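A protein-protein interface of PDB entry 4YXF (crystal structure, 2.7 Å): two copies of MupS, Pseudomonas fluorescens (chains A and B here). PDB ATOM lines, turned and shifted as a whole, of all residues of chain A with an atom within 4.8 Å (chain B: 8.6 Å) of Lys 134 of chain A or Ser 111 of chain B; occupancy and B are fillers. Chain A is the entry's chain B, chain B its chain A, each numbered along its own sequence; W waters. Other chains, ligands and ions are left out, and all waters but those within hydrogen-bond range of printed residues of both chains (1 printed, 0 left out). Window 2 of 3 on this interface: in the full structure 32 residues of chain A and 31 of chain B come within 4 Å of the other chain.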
ATOM      1  N   TYR A  78       5.119 -16.205  -1.000  1.00  0.00           N
ATOM      2  CA  TYR A  78       6.538 -16.445  -1.180  1.00  0.00           C
ATOM      3  C   TYR A  78       7.441 -16.164   0.023  1.00  0.00           C
ATOM      4  O   TYR A  78       8.465 -16.802   0.196  1.00  0.00           O
ATOM      5  CB  TYR A  78       7.009 -15.637  -2.356  1.00  0.00           C
ATOM      6  CG  TYR A  78       8.283 -16.132  -2.901  1.00  0.00           C
ATOM      7  CD1 TYR A  78       8.308 -17.240  -3.708  1.00  0.00           C
ATOM      8  CD2 TYR A  78       9.484 -15.495  -2.612  1.00  0.00           C
ATOM      9  CE1 TYR A  78       9.497 -17.720  -4.232  1.00  0.00           C
ATOM     10  CE2 TYR A  78      10.676 -15.960  -3.120  1.00  0.00           C
ATOM     11  CZ  TYR A  78      10.678 -17.080  -3.937  1.00  0.00           C
ATOM     12  OH  TYR A  78      11.863 -17.567  -4.486  1.00  0.00           O
ATOM     13  N   LEU A 130       5.337 -24.045  -8.081  1.00  0.00           N
ATOM     14  CA  LEU A 130       6.520 -23.467  -8.722  1.00  0.00           C
ATOM     15  C   LEU A 130       7.360 -22.694  -7.701  1.00  0.00           C
ATOM     16  O   LEU A 130       8.587 -22.795  -7.699  1.00  0.00           O
ATOM     17  CB  LEU A 130       6.161 -22.568  -9.913  1.00  0.00           C
ATOM     18  CG  LEU A 130       5.624 -23.259 -11.155  1.00  0.00           C
ATOM     19  CD1 LEU A 130       4.823 -22.350 -12.040  1.00  0.00           C
ATOM     20  CD2 LEU A 130       6.774 -23.815 -11.943  1.00  0.00           C
ATOM     21  N   TYR A 131       6.692 -21.919  -6.847  1.00  0.00           N
ATOM     22  CA  TYR A 131       7.376 -21.178  -5.802  1.00  0.00           C
ATOM     23  C   TYR A 131       8.238 -22.104  -4.983  1.00  0.00           C
ATOM     24  O   TYR A 131       9.465 -21.901  -4.919  1.00  0.00           O
ATOM     25  CB  TYR A 131       6.385 -20.500  -4.888  1.00  0.00           C
ATOM     26  CG  TYR A 131       5.794 -19.229  -5.467  1.00  0.00           C
ATOM     27  CD1 TYR A 131       6.188 -18.750  -6.724  1.00  0.00           C
ATOM     28  CD2 TYR A 131       4.858 -18.475  -4.730  1.00  0.00           C
ATOM     29  CE1 TYR A 131       5.647 -17.589  -7.247  1.00  0.00           C
ATOM     30  CE2 TYR A 131       4.314 -17.323  -5.243  1.00  0.00           C
ATOM     31  CZ  TYR A 131       4.713 -16.885  -6.497  1.00  0.00           C
ATOM     32  OH  TYR A 131       4.162 -15.716  -6.983  1.00  0.00           O
ATOM     33  N   LEU A 132       7.601 -23.133  -4.398  1.00  0.00           N
ATOM     34  CA  LEU A 132       8.310 -24.161  -3.584  1.00  0.00           C
ATOM     35  C   LEU A 132       9.445 -24.831  -4.382  1.00  0.00           C
ATOM     36  O   LEU A 132      10.554 -25.025  -3.871  1.00  0.00           O
ATOM     37  CB  LEU A 132       7.355 -25.231  -3.027  1.00  0.00           C
ATOM     38  CG  LEU A 132       7.961 -26.216  -2.017  1.00  0.00           C
ATOM     39  CD1 LEU A 132       8.629 -25.474  -0.847  1.00  0.00           C
ATOM     40  CD2 LEU A 132       6.926 -27.204  -1.467  1.00  0.00           C
ATOM     41  N   THR A 133       9.174 -25.171  -5.637  1.00  0.00           N
ATOM     42  CA  THR A 133      10.193 -25.784  -6.486  1.00  0.00           C
ATOM     43  C   THR A 133      11.425 -24.886  -6.602  1.00  0.00           C
ATOM     44  O   THR A 133      12.561 -25.344  -6.471  1.00  0.00           O
ATOM     45  CB  THR A 133       9.651 -26.081  -7.896  1.00  0.00           C
ATOM     46  OG1 THR A 133       8.647 -27.102  -7.819  1.00  0.00           O
ATOM     47  CG2 THR A 133      10.772 -26.546  -8.812  1.00  0.00           C
ATOM     48  N   LYS A 134      11.182 -23.603  -6.848  1.00  0.00           N
ATOM     49  CA  LYS A 134      12.252 -22.582  -6.984  1.00  0.00           C
ATOM     50  C   LYS A 134      13.110 -22.491  -5.704  1.00  0.00           C
ATOM     51  O   LYS A 134      14.329 -22.656  -5.778  1.00  0.00           O
ATOM     52  CB  LYS A 134      11.663 -21.229  -7.358  1.00  0.00           C
ATOM     53  CG  LYS A 134      12.693 -20.151  -7.633  1.00  0.00           C
ATOM     54  CD  LYS A 134      12.056 -18.770  -7.850  1.00  0.00           C
ATOM     55  CE  LYS A 134      13.052 -17.656  -7.494  1.00  0.00           C
ATOM     56  NZ  LYS A 134      14.424 -17.980  -8.031  1.00  0.00           N
ATOM     57  N   LEU A 135      12.462 -22.301  -4.560  1.00  0.00           N
ATOM     58  CA  LEU A 135      13.151 -22.284  -3.275  1.00  0.00           C
ATOM     59  C   LEU A 135      13.975 -23.551  -3.039  1.00  0.00           C
ATOM     60  O   LEU A 135      15.198 -23.485  -2.918  1.00  0.00           O
ATOM     61  CB  LEU A 135      12.149 -22.091  -2.134  1.00  0.00           C
ATOM     62  CG  LEU A 135      12.350 -20.852  -1.258  1.00  0.00           C
ATOM     63  CD1 LEU A 135      13.380 -19.918  -1.877  1.00  0.00           C
ATOM     64  CD2 LEU A 135      11.030 -20.130  -1.036  1.00  0.00           C
ATOM     65  N   VAL A 136      13.307 -24.701  -2.968  1.00  0.00           N
ATOM     66  CA  VAL A 136      14.003 -25.971  -2.680  1.00  0.00           C
ATOM     67  C   VAL A 136      15.154 -26.358  -3.649  1.00  0.00           C
ATOM     68  O   VAL A 136      16.272 -26.725  -3.283  1.00  0.00           O
ATOM     69  CB  VAL A 136      12.987 -27.071  -2.551  1.00  0.00           C
ATOM     70  CG1 VAL A 136      13.700 -28.362  -2.178  1.00  0.00           C
ATOM     71  CG2 VAL A 136      11.994 -26.669  -1.463  1.00  0.00           C
ATOM     72  N   THR A 137      14.890 -26.210  -4.913  1.00  0.00           N
ATOM     73  CA  THR A 137      15.893 -26.397  -5.942  1.00  0.00           C
ATOM     74  C   THR A 137      17.187 -25.622  -5.680  1.00  0.00           C
ATOM     75  O   THR A 137      18.296 -26.120  -5.923  1.00  0.00           O
ATOM     76  CB  THR A 137      15.132 -26.097  -7.206  1.00  0.00           C
ATOM     77  OG1 THR A 137      14.736 -27.362  -7.718  1.00  0.00           O
ATOM     78  CG2 THR A 137      15.795 -25.217  -8.180  1.00  0.00           C
ATOM     79  N   ALA A 138      17.085 -24.416  -5.137  1.00  0.00           N
ATOM     80  CA  ALA A 138      18.327 -23.668  -4.823  1.00  0.00           C
ATOM     81  C   ALA A 138      19.146 -24.350  -3.711  1.00  0.00           C
ATOM     82  O   ALA A 138      20.353 -24.520  -3.836  1.00  0.00           O
ATOM     83  CB  ALA A 138      17.979 -22.265  -4.435  1.00  0.00           C
ATOM     84  N   LEU A 141      20.758 -27.492  -5.403  1.00  0.00           N
ATOM     85  CA  LEU A 141      22.015 -27.082  -6.085  1.00  0.00           C
ATOM     86  C   LEU A 141      23.174 -26.932  -5.080  1.00  0.00           C
ATOM     87  O   LEU A 141      24.285 -27.365  -5.366  1.00  0.00           O
ATOM     88  CB  LEU A 141      21.853 -25.816  -6.945  1.00  0.00           C
ATOM     89  CG  LEU A 141      20.820 -26.032  -8.053  1.00  0.00           C
ATOM     90  CD1 LEU A 141      20.256 -24.730  -8.608  1.00  0.00           C
ATOM     91  CD2 LEU A 141      21.440 -26.879  -9.147  1.00  0.00           C
ATOM     92  N   GLY B 108      15.386 -18.759 -19.274  1.00  0.00           N
ATOM     93  CA  GLY B 108      16.088 -18.548 -18.023  1.00  0.00           C
ATOM     94  C   GLY B 108      15.880 -19.602 -16.961  1.00  0.00           C
ATOM     95  O   GLY B 108      14.740 -19.956 -16.634  1.00  0.00           O
ATOM     96  N   ILE B 109      16.994 -20.111 -16.418  1.00  0.00           N
ATOM     97  CA  ILE B 109      16.956 -21.087 -15.344  1.00  0.00           C
ATOM     98  C   ILE B 109      16.095 -20.609 -14.179  1.00  0.00           C
ATOM     99  O   ILE B 109      15.973 -19.412 -13.923  1.00  0.00           O
ATOM    100  CB  ILE B 109      18.348 -21.487 -14.909  1.00  0.00           C
ATOM    101  CG1 ILE B 109      19.120 -20.324 -14.282  1.00  0.00           C
ATOM    102  CG2 ILE B 109      19.129 -22.018 -16.083  1.00  0.00           C
ATOM    103  CD1 ILE B 109      20.529 -20.672 -13.849  1.00  0.00           C
ATOM    104  N   LEU B 110      15.462 -21.553 -13.506  1.00  0.00           N
ATOM    105  CA  LEU B 110      14.487 -21.264 -12.461  1.00  0.00           C
ATOM    106  C   LEU B 110      15.137 -20.529 -11.270  1.00  0.00           C
ATOM    107  O   LEU B 110      14.435 -19.875 -10.490  1.00  0.00           O
ATOM    108  CB  LEU B 110      13.860 -22.603 -11.982  1.00  0.00           C
ATOM    109  CG  LEU B 110      12.626 -22.612 -11.054  1.00  0.00           C
ATOM    110  CD1 LEU B 110      11.565 -21.539 -11.402  1.00  0.00           C
ATOM    111  CD2 LEU B 110      12.002 -23.995 -11.077  1.00  0.00           C
ATOM    112  N   SER B 111      16.465 -20.660 -11.106  1.00  0.00           N
ATOM    113  CA  SER B 111      17.219 -20.078  -9.961  1.00  0.00           C
ATOM    114  C   SER B 111      17.478 -18.564 -10.153  1.00  0.00           C
ATOM    115  O   SER B 111      17.228 -17.794  -9.236  1.00  0.00           O
ATOM    116  CB  SER B 111      18.517 -20.850  -9.734  1.00  0.00           C
ATOM    117  OG  SER B 111      19.120 -21.174 -10.986  1.00  0.00           O
ATOM    118  N   THR B 112      17.935 -18.149 -11.345  1.00  0.00           N
ATOM    119  CA  THR B 112      17.894 -16.735 -11.779  1.00  0.00           C
ATOM    120  C   THR B 112      16.438 -16.128 -11.941  1.00  0.00           C
ATOM    121  O   THR B 112      16.277 -14.961 -12.260  1.00  0.00           O
ATOM    122  CB  THR B 112      18.651 -16.553 -13.120  1.00  0.00           C
ATOM    123  N   MET B 113      15.375 -16.892 -11.734  1.00  0.00           N
ATOM    124  CA  MET B 113      14.079 -16.479 -12.270  1.00  0.00           C
ATOM    125  C   MET B 113      13.383 -15.524 -11.355  1.00  0.00           C
ATOM    126  O   MET B 113      13.059 -15.912 -10.246  1.00  0.00           O
ATOM    127  CB  MET B 113      13.158 -17.681 -12.351  1.00  0.00           C
ATOM    128  CG  MET B 113      11.805 -17.436 -12.949  1.00  0.00           C
ATOM    129  SD  MET B 113      11.953 -17.009 -14.683  1.00  0.00           S
ATOM    130  CE  MET B 113      12.313 -18.689 -15.236  1.00  0.00           C
ATOM    131  N   ARG B 114      13.090 -14.304 -11.801  1.00  0.00           N
ATOM    132  CA  ARG B 114      12.392 -13.377 -10.901  1.00  0.00           C
ATOM    133  C   ARG B 114      10.980 -13.833 -10.577  1.00  0.00           C
ATOM    134  O   ARG B 114      10.230 -14.184 -11.438  1.00  0.00           O
ATOM    135  CB  ARG B 114      12.437 -11.935 -11.410  1.00  0.00           C
ATOM    136  CG  ARG B 114      13.853 -11.369 -11.494  1.00  0.00           C
ATOM    137  CD  ARG B 114      13.868  -9.846 -11.625  1.00  0.00           C
ATOM    138  NE  ARG B 114      13.232  -9.387 -12.867  1.00  0.00           N
ATOM    139  CZ  ARG B 114      13.871  -8.890 -13.933  1.00  0.00           C
ATOM    140  NH1 ARG B 114      15.195  -8.750 -13.945  1.00  0.00           N
ATOM    141  NH2 ARG B 114      13.171  -8.515 -14.997  1.00  0.00           N
ATOM    142  N   VAL B 115      10.637 -13.853  -9.310  1.00  0.00           N
ATOM    143  CA  VAL B 115       9.316 -14.280  -8.850  1.00  0.00           C
ATOM    144  C   VAL B 115       8.194 -13.595  -9.606  1.00  0.00           C
ATOM    145  O   VAL B 115       7.159 -14.186  -9.785  1.00  0.00           O
ATOM    146  CB  VAL B 115       9.113 -13.882  -7.363  1.00  0.00           C
ATOM    147  CG1 VAL B 115       7.963 -14.635  -6.725  1.00  0.00           C
ATOM    148  CG2 VAL B 115      10.435 -13.984  -6.557  1.00  0.00           C
ATOM    149  N   ALA B 116       8.370 -12.340 -10.026  1.00  0.00           N
ATOM    150  CA  ALA B 116       7.296 -11.623 -10.757  1.00  0.00           C
ATOM    151  C   ALA B 116       7.160 -12.106 -12.209  1.00  0.00           C
ATOM    152  O   ALA B 116       6.083 -12.047 -12.782  1.00  0.00           O
ATOM    153  CB  ALA B 116       7.505 -10.137 -10.719  1.00  0.00           C
ATOM    154  N   ILE B 118       7.479 -15.282 -13.163  1.00  0.00           N
ATOM    155  CA  ILE B 118       6.635 -16.456 -13.024  1.00  0.00           C
ATOM    156  C   ILE B 118       5.164 -16.061 -13.013  1.00  0.00           C
ATOM    157  O   ILE B 118       4.323 -16.779 -13.575  1.00  0.00           O
ATOM    158  CB  ILE B 118       6.993 -17.204 -11.721  1.00  0.00           C
ATOM    159  CG1 ILE B 118       8.318 -17.937 -11.917  1.00  0.00           C
ATOM    160  CG2 ILE B 118       5.898 -18.132 -11.231  1.00  0.00           C
ATOM    161  CD1 ILE B 118       8.957 -18.353 -10.601  1.00  0.00           C
ATOM    162  N   GLY B 162      16.241 -24.355 -19.164  1.00  0.00           N
ATOM    163  CA  GLY B 162      15.952 -22.893 -19.228  1.00  0.00           C
ATOM    164  C   GLY B 162      14.534 -22.507 -19.704  1.00  0.00           C
ATOM    165  O   GLY B 162      14.200 -21.304 -19.674  1.00  0.00           O
ATOM    166  N   THR B 164      11.664 -23.985 -18.298  1.00  0.00           N
ATOM    167  CA  THR B 164      10.946 -24.501 -17.191  1.00  0.00           C
ATOM    168  C   THR B 164       9.527 -24.033 -17.042  1.00  0.00           C
ATOM    169  O   THR B 164       8.639 -24.803 -17.064  1.00  0.00           O
ATOM    170  CB  THR B 164      11.732 -24.157 -15.946  1.00  0.00           C
ATOM    171  OG1 THR B 164      12.999 -24.773 -16.037  1.00  0.00           O
ATOM    172  CG2 THR B 164      11.070 -24.670 -14.783  1.00  0.00           C
ATOM    173  N   VAL B 165       9.420 -22.716 -16.859  1.00  0.00           N
ATOM    174  CA  VAL B 165       8.060 -22.155 -16.627  1.00  0.00           C
ATOM    175  C   VAL B 165       7.245 -22.140 -17.931  1.00  0.00           C
ATOM    176  O   VAL B 165       5.987 -22.320 -17.946  1.00  0.00           O
ATOM    177  CB  VAL B 165       8.096 -20.732 -15.994  1.00  0.00           C
ATOM    178  CG1 VAL B 165       6.730 -20.068 -15.981  1.00  0.00           C
ATOM    179  CG2 VAL B 165       8.543 -20.798 -14.553  1.00  0.00           C
HETATM  180  O   HOH W   1      15.845 -15.133  -7.987  1.00  0.00           O
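NZ of Lys 134 of chain A lies within hydrogen-bond range of O of Leu 110 of chain B, at 3.1 Å. O of Ser 111 of chain B lies within hydrogen-bond range of NZ of Lys 134 of chain A (3.1 Å). O of Met 113 of chain B lies close to NZ of Lys 134 of chain A (3.3 Å).
The backbone carbonyl oxygen of Thr 133 of chain A sits close to the side-chain hydroxyl of Thr 137 of chain A.
Among the printed residues, pairs that only touch across the chains: Thr 133 of chain A with Leu 110 of chain B (3.6 Å), Tyr 131 of chain A with Val 115 of chain B (3.8 Å) and Tyr 78 of chain A with Val 115 of chain B (3.97 Å).
Lys 134 of chain A touches just these residues of chain B: Leu 110 (3.1 Å), Ser 111 (3.1 Å) and Met 113 (3.3 Å). Of chain A, only Lys 134 comes within 4 Å of Ser 111 of chain B. Of chain B, only Leu 110 (3.6 Å) comes within 4 Å of Thr 133 of chain A. Of the printed residues of chain A, Val 115 of chain B touches Tyr 78 and Tyr 131. Printed residues of chain A within 4 Å of Met 113 of chain B: Lys 134 (3.3 Å). Printed residues of chain A within 4 Å of Leu 110 of chain B: Thr 133 (3.6 Å) and Lys 134 (3.1 Å). Printed residues of chain B within 4 Å of Tyr 78 of chain A: Val 115. Leu 135 of chain A touches none of the printed residues of chain B. Ala 138 of chain A touches none of the printed residues of chain B. The nearest residue of chain A that does not touch Ser 111 of chain B is Leu 141 of chain A (4.4 Å). The nearest printed residue of chain B that does not touch Tyr 131 of chain A is Ile 118 of chain B (4.03 Å).
Of the 11 printed residues of chain A, 4 touch a printed residue of chain B. Of the 13 printed residues of chain B, 4 touch a printed residue of chain A. Hydrophobic or aromatic side chains of chain B that line the printed part of chain A: Leu 110 and Val 115.
No position is printed for both chains. Of the 6 pairs that touch across the chains among the printed residues, none has its exchanged pair printed and touching as well.
Water W1 lies within hydrogen-bond range of NZ of Lys 134 of chain A (3.2 Å) and O of Ser 111 of chain B (3.2 Å).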
